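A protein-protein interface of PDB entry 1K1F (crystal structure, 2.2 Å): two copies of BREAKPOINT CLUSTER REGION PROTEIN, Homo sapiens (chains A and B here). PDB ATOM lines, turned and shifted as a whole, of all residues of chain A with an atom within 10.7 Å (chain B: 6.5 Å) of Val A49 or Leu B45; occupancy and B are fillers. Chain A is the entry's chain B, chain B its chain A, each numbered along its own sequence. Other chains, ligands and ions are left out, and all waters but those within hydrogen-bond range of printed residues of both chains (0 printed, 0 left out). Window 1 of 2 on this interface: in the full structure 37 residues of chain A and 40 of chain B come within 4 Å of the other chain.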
ATOM      1  N   PHE A  15      31.490  19.098   6.741  1.00  0.00           N
ATOM      2  CA  PHE A  15      31.363  19.376   8.161  1.00  0.00           C
ATOM      3  C   PHE A  15      32.263  20.528   8.607  1.00  0.00           C
ATOM      4  O   PHE A  15      33.303  20.317   9.224  1.00  0.00           O
ATOM      5  CB  PHE A  15      31.689  18.110   8.963  1.00  0.00           C
ATOM      6  CG  PHE A  15      31.398  16.826   8.226  1.00  0.00           C
ATOM      7  CD1 PHE A  15      32.355  16.264   7.377  1.00  0.00           C
ATOM      8  CD2 PHE A  15      30.173  16.178   8.373  1.00  0.00           C
ATOM      9  CE1 PHE A  15      32.096  15.076   6.688  1.00  0.00           C
ATOM     10  CE2 PHE A  15      29.905  14.989   7.686  1.00  0.00           C
ATOM     11  CZ  PHE A  15      30.871  14.438   6.843  1.00  0.00           C
ATOM     12  N   SER A  41      33.343   2.892  15.507  1.00  0.00           N
ATOM     13  CA  SER A  41      32.602   4.070  15.903  1.00  0.00           C
ATOM     14  C   SER A  41      31.275   4.092  15.161  1.00  0.00           C
ATOM     15  O   SER A  41      30.235   4.317  15.759  1.00  0.00           O
ATOM     16  CB  SER A  41      33.403   5.338  15.597  1.00  0.00           C
ATOM     17  OG  SER A  41      34.541   5.411  16.444  1.00  0.00           O
ATOM     18  N   ILE A  42      31.308   3.838  13.858  1.00  0.00           N
ATOM     19  CA  ILE A  42      30.072   3.832  13.073  1.00  0.00           C
ATOM     20  C   ILE A  42      29.025   2.891  13.658  1.00  0.00           C
ATOM     21  O   ILE A  42      27.900   3.300  13.979  1.00  0.00           O
ATOM     22  CB  ILE A  42      30.336   3.402  11.609  1.00  0.00           C
ATOM     23  CG1 ILE A  42      31.243   4.432  10.921  1.00  0.00           C
ATOM     24  CG2 ILE A  42      29.025   3.248  10.865  1.00  0.00           C
ATOM     25  CD1 ILE A  42      31.667   4.035   9.513  1.00  0.00           C
ATOM     26  N   ARG A  43      29.389   1.622  13.792  1.00  0.00           N
ATOM     27  CA  ARG A  43      28.445   0.655  14.326  1.00  0.00           C
ATOM     28  C   ARG A  43      27.937   1.074  15.692  1.00  0.00           C
ATOM     29  O   ARG A  43      26.846   0.692  16.087  1.00  0.00           O
ATOM     30  CB  ARG A  43      29.079  -0.749  14.377  1.00  0.00           C
ATOM     31  CG  ARG A  43      29.308  -1.320  12.975  1.00  0.00           C
ATOM     32  CD  ARG A  43      29.409  -2.840  12.937  1.00  0.00           C
ATOM     33  NE  ARG A  43      29.001  -3.350  11.622  1.00  0.00           N
ATOM     34  CZ  ARG A  43      29.142  -4.610  11.219  1.00  0.00           C
ATOM     35  NH1 ARG A  43      29.686  -5.513  12.028  1.00  0.00           N
ATOM     36  NH2 ARG A  43      28.743  -4.966  10.003  1.00  0.00           N
ATOM     37  N   ARG A  44      28.718   1.885  16.399  1.00  0.00           N
ATOM     38  CA  ARG A  44      28.333   2.342  17.736  1.00  0.00           C
ATOM     39  C   ARG A  44      27.423   3.562  17.697  1.00  0.00           C
ATOM     40  O   ARG A  44      26.406   3.629  18.401  1.00  0.00           O
ATOM     41  CB  ARG A  44      29.578   2.675  18.550  1.00  0.00           C
ATOM     42  CG  ARG A  44      29.270   3.099  19.976  1.00  0.00           C
ATOM     43  CD  ARG A  44      30.336   2.578  20.937  1.00  0.00           C
ATOM     44  NE  ARG A  44      29.795   2.428  22.288  1.00  0.00           N
ATOM     45  CZ  ARG A  44      30.229   1.530  23.172  1.00  0.00           C
ATOM     46  NH1 ARG A  44      31.218   0.697  22.848  1.00  0.00           N
ATOM     47  NH2 ARG A  44      29.667   1.452  24.377  1.00  0.00           N
ATOM     48  N   LEU A  45      27.804   4.534  16.884  1.00  0.00           N
ATOM     49  CA  LEU A  45      27.016   5.750  16.751  1.00  0.00           C
ATOM     50  C   LEU A  45      25.690   5.422  16.081  1.00  0.00           C
ATOM     51  O   LEU A  45      24.679   6.078  16.339  1.00  0.00           O
ATOM     52  CB  LEU A  45      27.777   6.778  15.909  1.00  0.00           C
ATOM     53  CG  LEU A  45      28.678   7.794  16.624  1.00  0.00           C
ATOM     54  CD1 LEU A  45      29.257   7.186  17.869  1.00  0.00           C
ATOM     55  CD2 LEU A  45      29.781   8.241  15.687  1.00  0.00           C
ATOM     56  N   GLU A  46      25.703   4.406  15.220  1.00  0.00           N
ATOM     57  CA  GLU A  46      24.496   4.018  14.504  1.00  0.00           C
ATOM     58  C   GLU A  46      23.462   3.451  15.453  1.00  0.00           C
ATOM     59  O   GLU A  46      22.280   3.759  15.319  1.00  0.00           O
ATOM     60  CB  GLU A  46      24.821   2.992  13.422  1.00  0.00           C
ATOM     61  CG  GLU A  46      23.710   2.750  12.415  1.00  0.00           C
ATOM     62  CD  GLU A  46      23.111   4.037  11.889  1.00  0.00           C
ATOM     63  OE1 GLU A  46      22.061   4.455  12.425  1.00  0.00           O
ATOM     64  OE2 GLU A  46      23.689   4.639  10.953  1.00  0.00           O
ATOM     65  N   GLN A  47      23.899   2.641  16.417  1.00  0.00           N
ATOM     66  CA  GLN A  47      22.977   2.050  17.372  1.00  0.00           C
ATOM     67  C   GLN A  47      22.486   3.106  18.351  1.00  0.00           C
ATOM     68  O   GLN A  47      21.368   3.026  18.857  1.00  0.00           O
ATOM     69  CB  GLN A  47      23.640   0.909  18.147  1.00  0.00           C
ATOM     70  CG  GLN A  47      22.672   0.214  19.108  1.00  0.00           C
ATOM     71  CD  GLN A  47      23.314  -0.899  19.917  1.00  0.00           C
ATOM     72  OE1 GLN A  47      24.257  -0.671  20.676  1.00  0.00           O
ATOM     73  NE2 GLN A  47      22.794  -2.116  19.765  1.00  0.00           N
ATOM     74  N   GLU A  48      23.331   4.088  18.641  1.00  0.00           N
ATOM     75  CA  GLU A  48      22.915   5.142  19.546  1.00  0.00           C
ATOM     76  C   GLU A  48      21.900   6.059  18.879  1.00  0.00           C
ATOM     77  O   GLU A  48      21.070   6.650  19.556  1.00  0.00           O
ATOM     78  CB  GLU A  48      24.128   5.918  20.038  1.00  0.00           C
ATOM     79  CG  GLU A  48      25.178   4.964  20.540  1.00  0.00           C
ATOM     80  CD  GLU A  48      25.817   5.413  21.823  1.00  0.00           C
ATOM     81  OE1 GLU A  48      25.092   5.560  22.832  1.00  0.00           O
ATOM     82  OE2 GLU A  48      27.046   5.609  21.818  1.00  0.00           O
ATOM     83  N   VAL A  49      21.938   6.181  17.555  1.00  0.00           N
ATOM     84  CA  VAL A  49      20.950   7.044  16.898  1.00  0.00           C
ATOM     85  C   VAL A  49      19.613   6.314  16.922  1.00  0.00           C
ATOM     86  O   VAL A  49      18.555   6.932  17.084  1.00  0.00           O
ATOM     87  CB  VAL A  49      21.315   7.351  15.429  1.00  0.00           C
ATOM     88  CG1 VAL A  49      20.327   8.386  14.867  1.00  0.00           C
ATOM     89  CG2 VAL A  49      22.742   7.893  15.351  1.00  0.00           C
ATOM     90  N   ASN A  50      19.670   4.990  16.776  1.00  0.00           N
ATOM     91  CA  ASN A  50      18.463   4.160  16.788  1.00  0.00           C
ATOM     92  C   ASN A  50      17.839   4.176  18.171  1.00  0.00           C
ATOM     93  O   ASN A  50      16.623   4.194  18.320  1.00  0.00           O
ATOM     94  CB  ASN A  50      18.802   2.716  16.404  1.00  0.00           C
ATOM     95  CG  ASN A  50      19.066   2.552  14.932  1.00  0.00           C
ATOM     96  OD1 ASN A  50      19.629   1.536  14.498  1.00  0.00           O
ATOM     97  ND2 ASN A  50      18.651   3.530  14.147  1.00  0.00           N
ATOM     98  N   GLN A  51      18.691   4.142  19.185  1.00  0.00           N
ATOM     99  CA  GLN A  51      18.235   4.172  20.558  1.00  0.00           C
ATOM    100  C   GLN A  51      17.539   5.500  20.826  1.00  0.00           C
ATOM    101  O   GLN A  51      16.527   5.560  21.534  1.00  0.00           O
ATOM    102  CB  GLN A  51      19.431   4.022  21.489  1.00  0.00           C
ATOM    103  CG  GLN A  51      19.999   2.613  21.593  1.00  0.00           C
ATOM    104  CD  GLN A  51      21.357   2.610  22.258  1.00  0.00           C
ATOM    105  OE1 GLN A  51      21.567   3.283  23.268  1.00  0.00           O
ATOM    106  NE2 GLN A  51      22.292   1.869  21.687  1.00  0.00           N
ATOM    107  N   GLU A  52      18.085   6.572  20.263  1.00  0.00           N
ATOM    108  CA  GLU A  52      17.516   7.911  20.448  1.00  0.00           C
ATOM    109  C   GLU A  52      16.159   7.999  19.735  1.00  0.00           C
ATOM    110  O   GLU A  52      15.157   8.519  20.266  1.00  0.00           O
ATOM    111  CB  GLU A  52      18.496   8.942  19.877  1.00  0.00           C
ATOM    112  CG  GLU A  52      18.521  10.220  20.633  1.00  0.00           C
ATOM    113  CD  GLU A  52      19.038  10.027  22.033  1.00  0.00           C
ATOM    114  OE1 GLU A  52      20.232   9.709  22.179  1.00  0.00           O
ATOM    115  OE2 GLU A  52      18.253  10.190  22.981  1.00  0.00           O
ATOM    116  N   ARG A  53      16.127   7.468  18.522  1.00  0.00           N
ATOM    117  CA  ARG A  53      14.904   7.458  17.724  1.00  0.00           C
ATOM    118  C   ARG A  53      13.815   6.684  18.480  1.00  0.00           C
ATOM    119  O   ARG A  53      12.640   7.055  18.467  1.00  0.00           O
ATOM    120  CB  ARG A  53      15.189   6.799  16.369  1.00  0.00           C
ATOM    121  CG  ARG A  53      16.023   7.671  15.400  1.00  0.00           C
ATOM    122  CD  ARG A  53      16.367   6.897  14.110  1.00  0.00           C
ATOM    123  NE  ARG A  53      17.071   7.688  13.091  1.00  0.00           N
ATOM    124  CZ  ARG A  53      16.521   8.678  12.377  1.00  0.00           C
ATOM    125  NH1 ARG A  53      15.253   9.016  12.559  1.00  0.00           N
ATOM    126  NH2 ARG A  53      17.235   9.332  11.466  1.00  0.00           N
ATOM    127  N   PHE A  54      14.213   5.610  19.143  1.00  0.00           N
ATOM    128  CA  PHE A  54      13.278   4.800  19.908  1.00  0.00           C
ATOM    129  C   PHE A  54      12.752   5.625  21.074  1.00  0.00           C
ATOM    130  O   PHE A  54      11.550   5.630  21.371  1.00  0.00           O
ATOM    131  CB  PHE A  54      13.996   3.559  20.445  1.00  0.00           C
ATOM    132  CG  PHE A  54      13.191   2.776  21.441  1.00  0.00           C
ATOM    133  CD1 PHE A  54      12.017   2.157  21.052  1.00  0.00           C
ATOM    134  CD2 PHE A  54      13.612   2.651  22.762  1.00  0.00           C
ATOM    135  CE1 PHE A  54      11.256   1.410  21.965  1.00  0.00           C
ATOM    136  CE2 PHE A  54      12.864   1.907  23.680  1.00  0.00           C
ATOM    137  CZ  PHE A  54      11.679   1.286  23.272  1.00  0.00           C
ATOM    138  N   ARG A  55      13.667   6.306  21.754  1.00  0.00           N
ATOM    139  CA  ARG A  55      13.295   7.149  22.888  1.00  0.00           C
ATOM    140  C   ARG A  55      12.370   8.270  22.437  1.00  0.00           C
ATOM    141  O   ARG A  55      11.424   8.602  23.142  1.00  0.00           O
ATOM    142  CB  ARG A  55      14.536   7.752  23.556  1.00  0.00           C
ATOM    143  CG  ARG A  55      14.315   9.155  24.141  1.00  0.00           C
ATOM    144  CD  ARG A  55      15.253   9.409  25.328  1.00  0.00           C
ATOM    145  NE  ARG A  55      16.655   9.090  25.041  1.00  0.00           N
ATOM    146  CZ  ARG A  55      17.600   9.039  25.980  1.00  0.00           C
ATOM    147  NH1 ARG A  55      17.280   9.292  27.242  1.00  0.00           N
ATOM    148  NH2 ARG A  55      18.850   8.711  25.672  1.00  0.00           N
ATOM    149  N   MET A  56      12.650   8.871  21.280  1.00  0.00           N
ATOM    150  CA  MET A  56      11.813   9.950  20.747  1.00  0.00           C
ATOM    151  C   MET A  56      10.423   9.411  20.440  1.00  0.00           C
ATOM    152  O   MET A  56       9.394  10.010  20.792  1.00  0.00           O
ATOM    153  CB  MET A  56      12.427  10.519  19.475  1.00  0.00           C
ATOM    154  CG  MET A  56      11.562  11.565  18.776  1.00  0.00           C
ATOM    155  SD  MET A  56      12.534  12.498  17.394  1.00  0.00           S
ATOM    156  CE  MET A  56      13.894  13.220  18.544  1.00  0.00           C
ATOM    157  N   ILE A  57      10.383   8.282  19.750  1.00  0.00           N
ATOM    158  CA  ILE A  57       9.092   7.690  19.461  1.00  0.00           C
ATOM    159  C   ILE A  57       8.348   7.570  20.790  1.00  0.00           C
ATOM    160  O   ILE A  57       7.309   8.179  20.944  1.00  0.00           O
ATOM    161  CB  ILE A  57       9.285   6.345  18.781  1.00  0.00           C
ATOM    162  CG1 ILE A  57       9.900   6.576  17.416  1.00  0.00           C
ATOM    163  CG2 ILE A  57       7.946   5.656  18.565  1.00  0.00           C
ATOM    164  CD1 ILE A  57      10.564   5.362  16.888  1.00  0.00           C
ATOM    165  N   ALA B  40      17.948  17.058  19.481  1.00  0.00           N
ATOM    166  CA  ALA B  40      19.241  17.712  19.297  1.00  0.00           C
ATOM    167  C   ALA B  40      20.328  16.651  19.202  1.00  0.00           C
ATOM    168  O   ALA B  40      21.280  16.769  18.426  1.00  0.00           O
ATOM    169  CB  ALA B  40      19.524  18.631  20.467  1.00  0.00           C
ATOM    170  N   SER B  41      20.164  15.613  20.013  1.00  0.00           N
ATOM    171  CA  SER B  41      21.105  14.508  20.081  1.00  0.00           C
ATOM    172  C   SER B  41      21.134  13.682  18.804  1.00  0.00           C
ATOM    173  O   SER B  41      22.189  13.246  18.358  1.00  0.00           O
ATOM    174  CB  SER B  41      20.746  13.619  21.265  1.00  0.00           C
ATOM    175  OG  SER B  41      20.817  12.257  20.897  1.00  0.00           O
ATOM    176  N   ILE B  42      19.975  13.439  18.224  1.00  0.00           N
ATOM    177  CA  ILE B  42      19.925  12.681  16.984  1.00  0.00           C
ATOM    178  C   ILE B  42      20.716  13.421  15.898  1.00  0.00           C
ATOM    179  O   ILE B  42      21.368  12.783  15.079  1.00  0.00           O
ATOM    180  CB  ILE B  42      18.473  12.472  16.510  1.00  0.00           C
ATOM    181  CG1 ILE B  42      17.791  11.427  17.385  1.00  0.00           C
ATOM    182  CG2 ILE B  42      18.448  11.991  15.064  1.00  0.00           C
ATOM    183  CD1 ILE B  42      16.329  11.235  17.058  1.00  0.00           C
ATOM    184  N   ARG B  43      20.664  14.755  15.907  1.00  0.00           N
ATOM    185  CA  ARG B  43      21.384  15.566  14.916  1.00  0.00           C
ATOM    186  C   ARG B  43      22.901  15.518  15.127  1.00  0.00           C
ATOM    187  O   ARG B  43      23.679  15.533  14.169  1.00  0.00           O
ATOM    188  CB  ARG B  43      20.911  17.031  14.965  1.00  0.00           C
ATOM    189  CG  ARG B  43      21.760  18.011  14.124  1.00  0.00           C
ATOM    190  CD  ARG B  43      21.296  19.468  14.236  1.00  0.00           C
ATOM    191  NE  ARG B  43      22.425  20.397  14.131  1.00  0.00           N
ATOM    192  CZ  ARG B  43      22.331  21.727  14.161  1.00  0.00           C
ATOM    193  NH1 ARG B  43      21.147  22.318  14.289  1.00  0.00           N
ATOM    194  NH2 ARG B  43      23.430  22.473  14.071  1.00  0.00           N
ATOM    195  N   ARG B  44      23.311  15.476  16.391  1.00  0.00           N
ATOM    196  CA  ARG B  44      24.721  15.422  16.745  1.00  0.00           C
ATOM    197  C   ARG B  44      25.318  14.097  16.279  1.00  0.00           C
ATOM    198  O   ARG B  44      26.441  14.066  15.765  1.00  0.00           O
ATOM    199  CB  ARG B  44      24.877  15.524  18.262  1.00  0.00           C
ATOM    200  CG  ARG B  44      25.944  16.490  18.729  1.00  0.00           C
ATOM    201  CD  ARG B  44      25.624  17.894  18.243  1.00  0.00           C
ATOM    202  NE  ARG B  44      25.783  18.896  19.295  1.00  0.00           N
ATOM    203  CZ  ARG B  44      25.464  20.181  19.160  1.00  0.00           C
ATOM    204  NH1 ARG B  44      24.964  20.631  18.013  1.00  0.00           N
ATOM    205  NH2 ARG B  44      25.654  21.020  20.172  1.00  0.00           N
ATOM    206  N   LEU B  45      24.555  13.015  16.475  1.00  0.00           N
ATOM    207  CA  LEU B  45      24.967  11.652  16.111  1.00  0.00           C
ATOM    208  C   LEU B  45      24.903  11.338  14.617  1.00  0.00           C
ATOM    209  O   LEU B  45      25.740  10.590  14.117  1.00  0.00           O
ATOM    210  CB  LEU B  45      24.120  10.609  16.870  1.00  0.00           C
ATOM    211  CG  LEU B  45      24.222  10.553  18.401  1.00  0.00           C
ATOM    212  CD1 LEU B  45      23.056   9.760  18.956  1.00  0.00           C
ATOM    213  CD2 LEU B  45      25.556   9.927  18.833  1.00  0.00           C
ATOM    214  N   GLU B  46      23.901  11.866  13.918  1.00  0.00           N
ATOM    215  CA  GLU B  46      23.774  11.631  12.481  1.00  0.00           C
ATOM    216  C   GLU B  46      24.939  12.289  11.738  1.00  0.00           C
ATOM    217  O   GLU B  46      25.388  11.776  10.712  1.00  0.00           O
ATOM    218  CB  GLU B  46      22.447  12.185  11.934  1.00  0.00           C
ATOM    219  CG  GLU B  46      21.198  11.431  12.376  1.00  0.00           C
ATOM    220  CD  GLU B  46      19.916  12.072  11.858  1.00  0.00           C
ATOM    221  OE1 GLU B  46      19.795  13.313  11.956  1.00  0.00           O
ATOM    222  OE2 GLU B  46      19.029  11.340  11.360  1.00  0.00           O
ATOM    223  N   GLN B  47      25.416  13.426  12.243  1.00  0.00           N
ATOM    224  CA  GLN B  47      26.534  14.095  11.587  1.00  0.00           C
ATOM    225  C   GLN B  47      27.788  13.293  11.874  1.00  0.00           C
ATOM    226  O   GLN B  47      28.599  13.054  10.977  1.00  0.00           O
ATOM    227  CB  GLN B  47      26.731  15.530  12.089  1.00  0.00           C
ATOM    228  CG  GLN B  47      27.913  16.225  11.400  1.00  0.00           C
ATOM    229  CD  GLN B  47      28.228  17.605  11.960  1.00  0.00           C
ATOM    230  OE1 GLN B  47      28.535  17.756  13.152  1.00  0.00           O
ATOM    231  NE2 GLN B  47      28.167  18.625  11.096  1.00  0.00           N
ATOM    232  N   GLU B  48      27.949  12.877  13.131  1.00  0.00           N
ATOM    233  CA  GLU B  48      29.110  12.073  13.495  1.00  0.00           C
ATOM    234  C   GLU B  48      29.115  10.791  12.666  1.00  0.00           C
ATOM    235  O   GLU B  48      30.167  10.359  12.208  1.00  0.00           O
ATOM    236  CB  GLU B  48      29.103  11.738  14.988  1.00  0.00           C
ATOM    237  CG  GLU B  48      29.162  12.958  15.883  1.00  0.00           C
ATOM    238  CD  GLU B  48      29.966  12.712  17.146  1.00  0.00           C
ATOM    239  OE1 GLU B  48      31.178  12.447  17.022  1.00  0.00           O
ATOM    240  OE2 GLU B  48      29.396  12.783  18.256  1.00  0.00           O
ATOM    241  N   VAL B  49      27.944  10.192  12.459  1.00  0.00           N
ATOM    242  CA  VAL B  49      27.867   8.961  11.672  1.00  0.00           C
ATOM    243  C   VAL B  49      28.343   9.237  10.256  1.00  0.00           C
ATOM    244  O   VAL B  49      28.986   8.382   9.629  1.00  0.00           O
ATOM    245  CB  VAL B  49      26.433   8.376  11.598  1.00  0.00           C
ATOM    246  CG1 VAL B  49      26.382   7.246  10.559  1.00  0.00           C
ATOM    247  CG2 VAL B  49      26.011   7.833  12.947  1.00  0.00           C
ATOM    248  N   ASN B  50      28.025  10.430   9.756  1.00  0.00           N
ATOM    249  CA  ASN B  50      28.425  10.817   8.411  1.00  0.00           C
ATOM    250  C   ASN B  50      29.903  11.151   8.306  1.00  0.00           C
ATOM    251  O   ASN B  50      30.507  10.922   7.271  1.00  0.00           O
ATOM    252  CB  ASN B  50      27.597  12.004   7.912  1.00  0.00           C
ATOM    253  CG  ASN B  50      26.136  11.659   7.759  1.00  0.00           C
ATOM    254  OD1 ASN B  50      25.788  10.532   7.401  1.00  0.00           O
ATOM    255  ND2 ASN B  50      25.261  12.638   8.010  1.00  0.00           N
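The side-chain carboxylate of Glu B46 lies within salt-bridge range of the guanidinium group of Arg A53.
OG of Ser B41 lies within hydrogen-bond range of OE1 of Glu A52, 2.9 Å away.
The backbone carbonyl oxygen (O) of Glu B46 is in hydrogen-bond range of the side-chain amide nitrogen (ND2) of Asn B50, 2.8 Å away.
The guanidinium group (NE) of Arg A55 is in salt-bridge range of the side-chain carboxylate (OE2) of Glu A52 (2.8 Å).
Among the printed residues, merely in contact across the chains: Val A49 with Leu B45 (3.4 Å), Met A56 with Ile B42 (3.5 Å), Glu A52 with Ile B42 (3.5 Å), Phe A15 with Asn B50 (3.6 Å), Leu A45 with Val B49 (3.6 Å), Leu A45 with Glu B48 (3.6 Å), Glu A48 with Leu B45 (3.7 Å), Glu A46 with Val B49 (3.8 Å), Phe A15 with Gln B47 (3.8 Å) and Arg A53 with Ile B42 (3.9 Å).
Of the printed residues of chain B, Glu A48 touches Leu B45 (3.7 Å).
Val A49 touches one residue of chain B.
Printed residues of chain B within 4 Å of Glu A52: Ser B41 and Ile B42.
Of the printed residues of chain B, Arg A53 touches Ile B42 (3.9 Å) and Glu B46 (2.7 Å).
Of chain A, only Glu A52 (2.9 Å) comes within 4 Å of Ser B41.
Of chain A, only Glu A52, Arg A53 and Met A56 come within 4 Å of Ile B42.
Of chain A, only Glu A48 and Val A49 come within 4 Å of Leu B45.
Glu B46 touches one residue of chain A.
Printed residues of chain A within 4 Å of Gln B47: Phe A15.
Printed residues of chain A within 4 Å of Asn B50: Phe A15.
The nearest residue of chain A that does not touch Leu B45 is Glu A52 (4.3 Å).
Printed residues of chain A that touch a printed residue of chain B: Phe A15, Leu A45, Glu A46, Glu A48, Val A49, Glu A52, Arg A53 and Met A56.
Hydrophobic or aromatic side chains of chain A that line the printed part of chain B: Phe A15, Leu A45, Val A49 and Met A56.
Among the printed residues, 12 pairs touch across the chains.
Among the printed residues, Asp or Glu carboxylates within 4 Å of a Lys or Arg side-chain nitrogen of the other chain: Arg A53 with Glu B46.
Leu A45 touches Glu B48, and with the chains exchanged Glu A48 touches Leu B45.
Leu A45 touches Val B49, and with the chains exchanged Val A49 touches Leu B45.
Glu A46 touches Val B49, but with the chains exchanged Val A49 does not touch Glu B46 (4.03 Å).
Of the 12 pairs that touch across the chains among the printed residues, 4 have their exchanged pair printed and touching as well.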
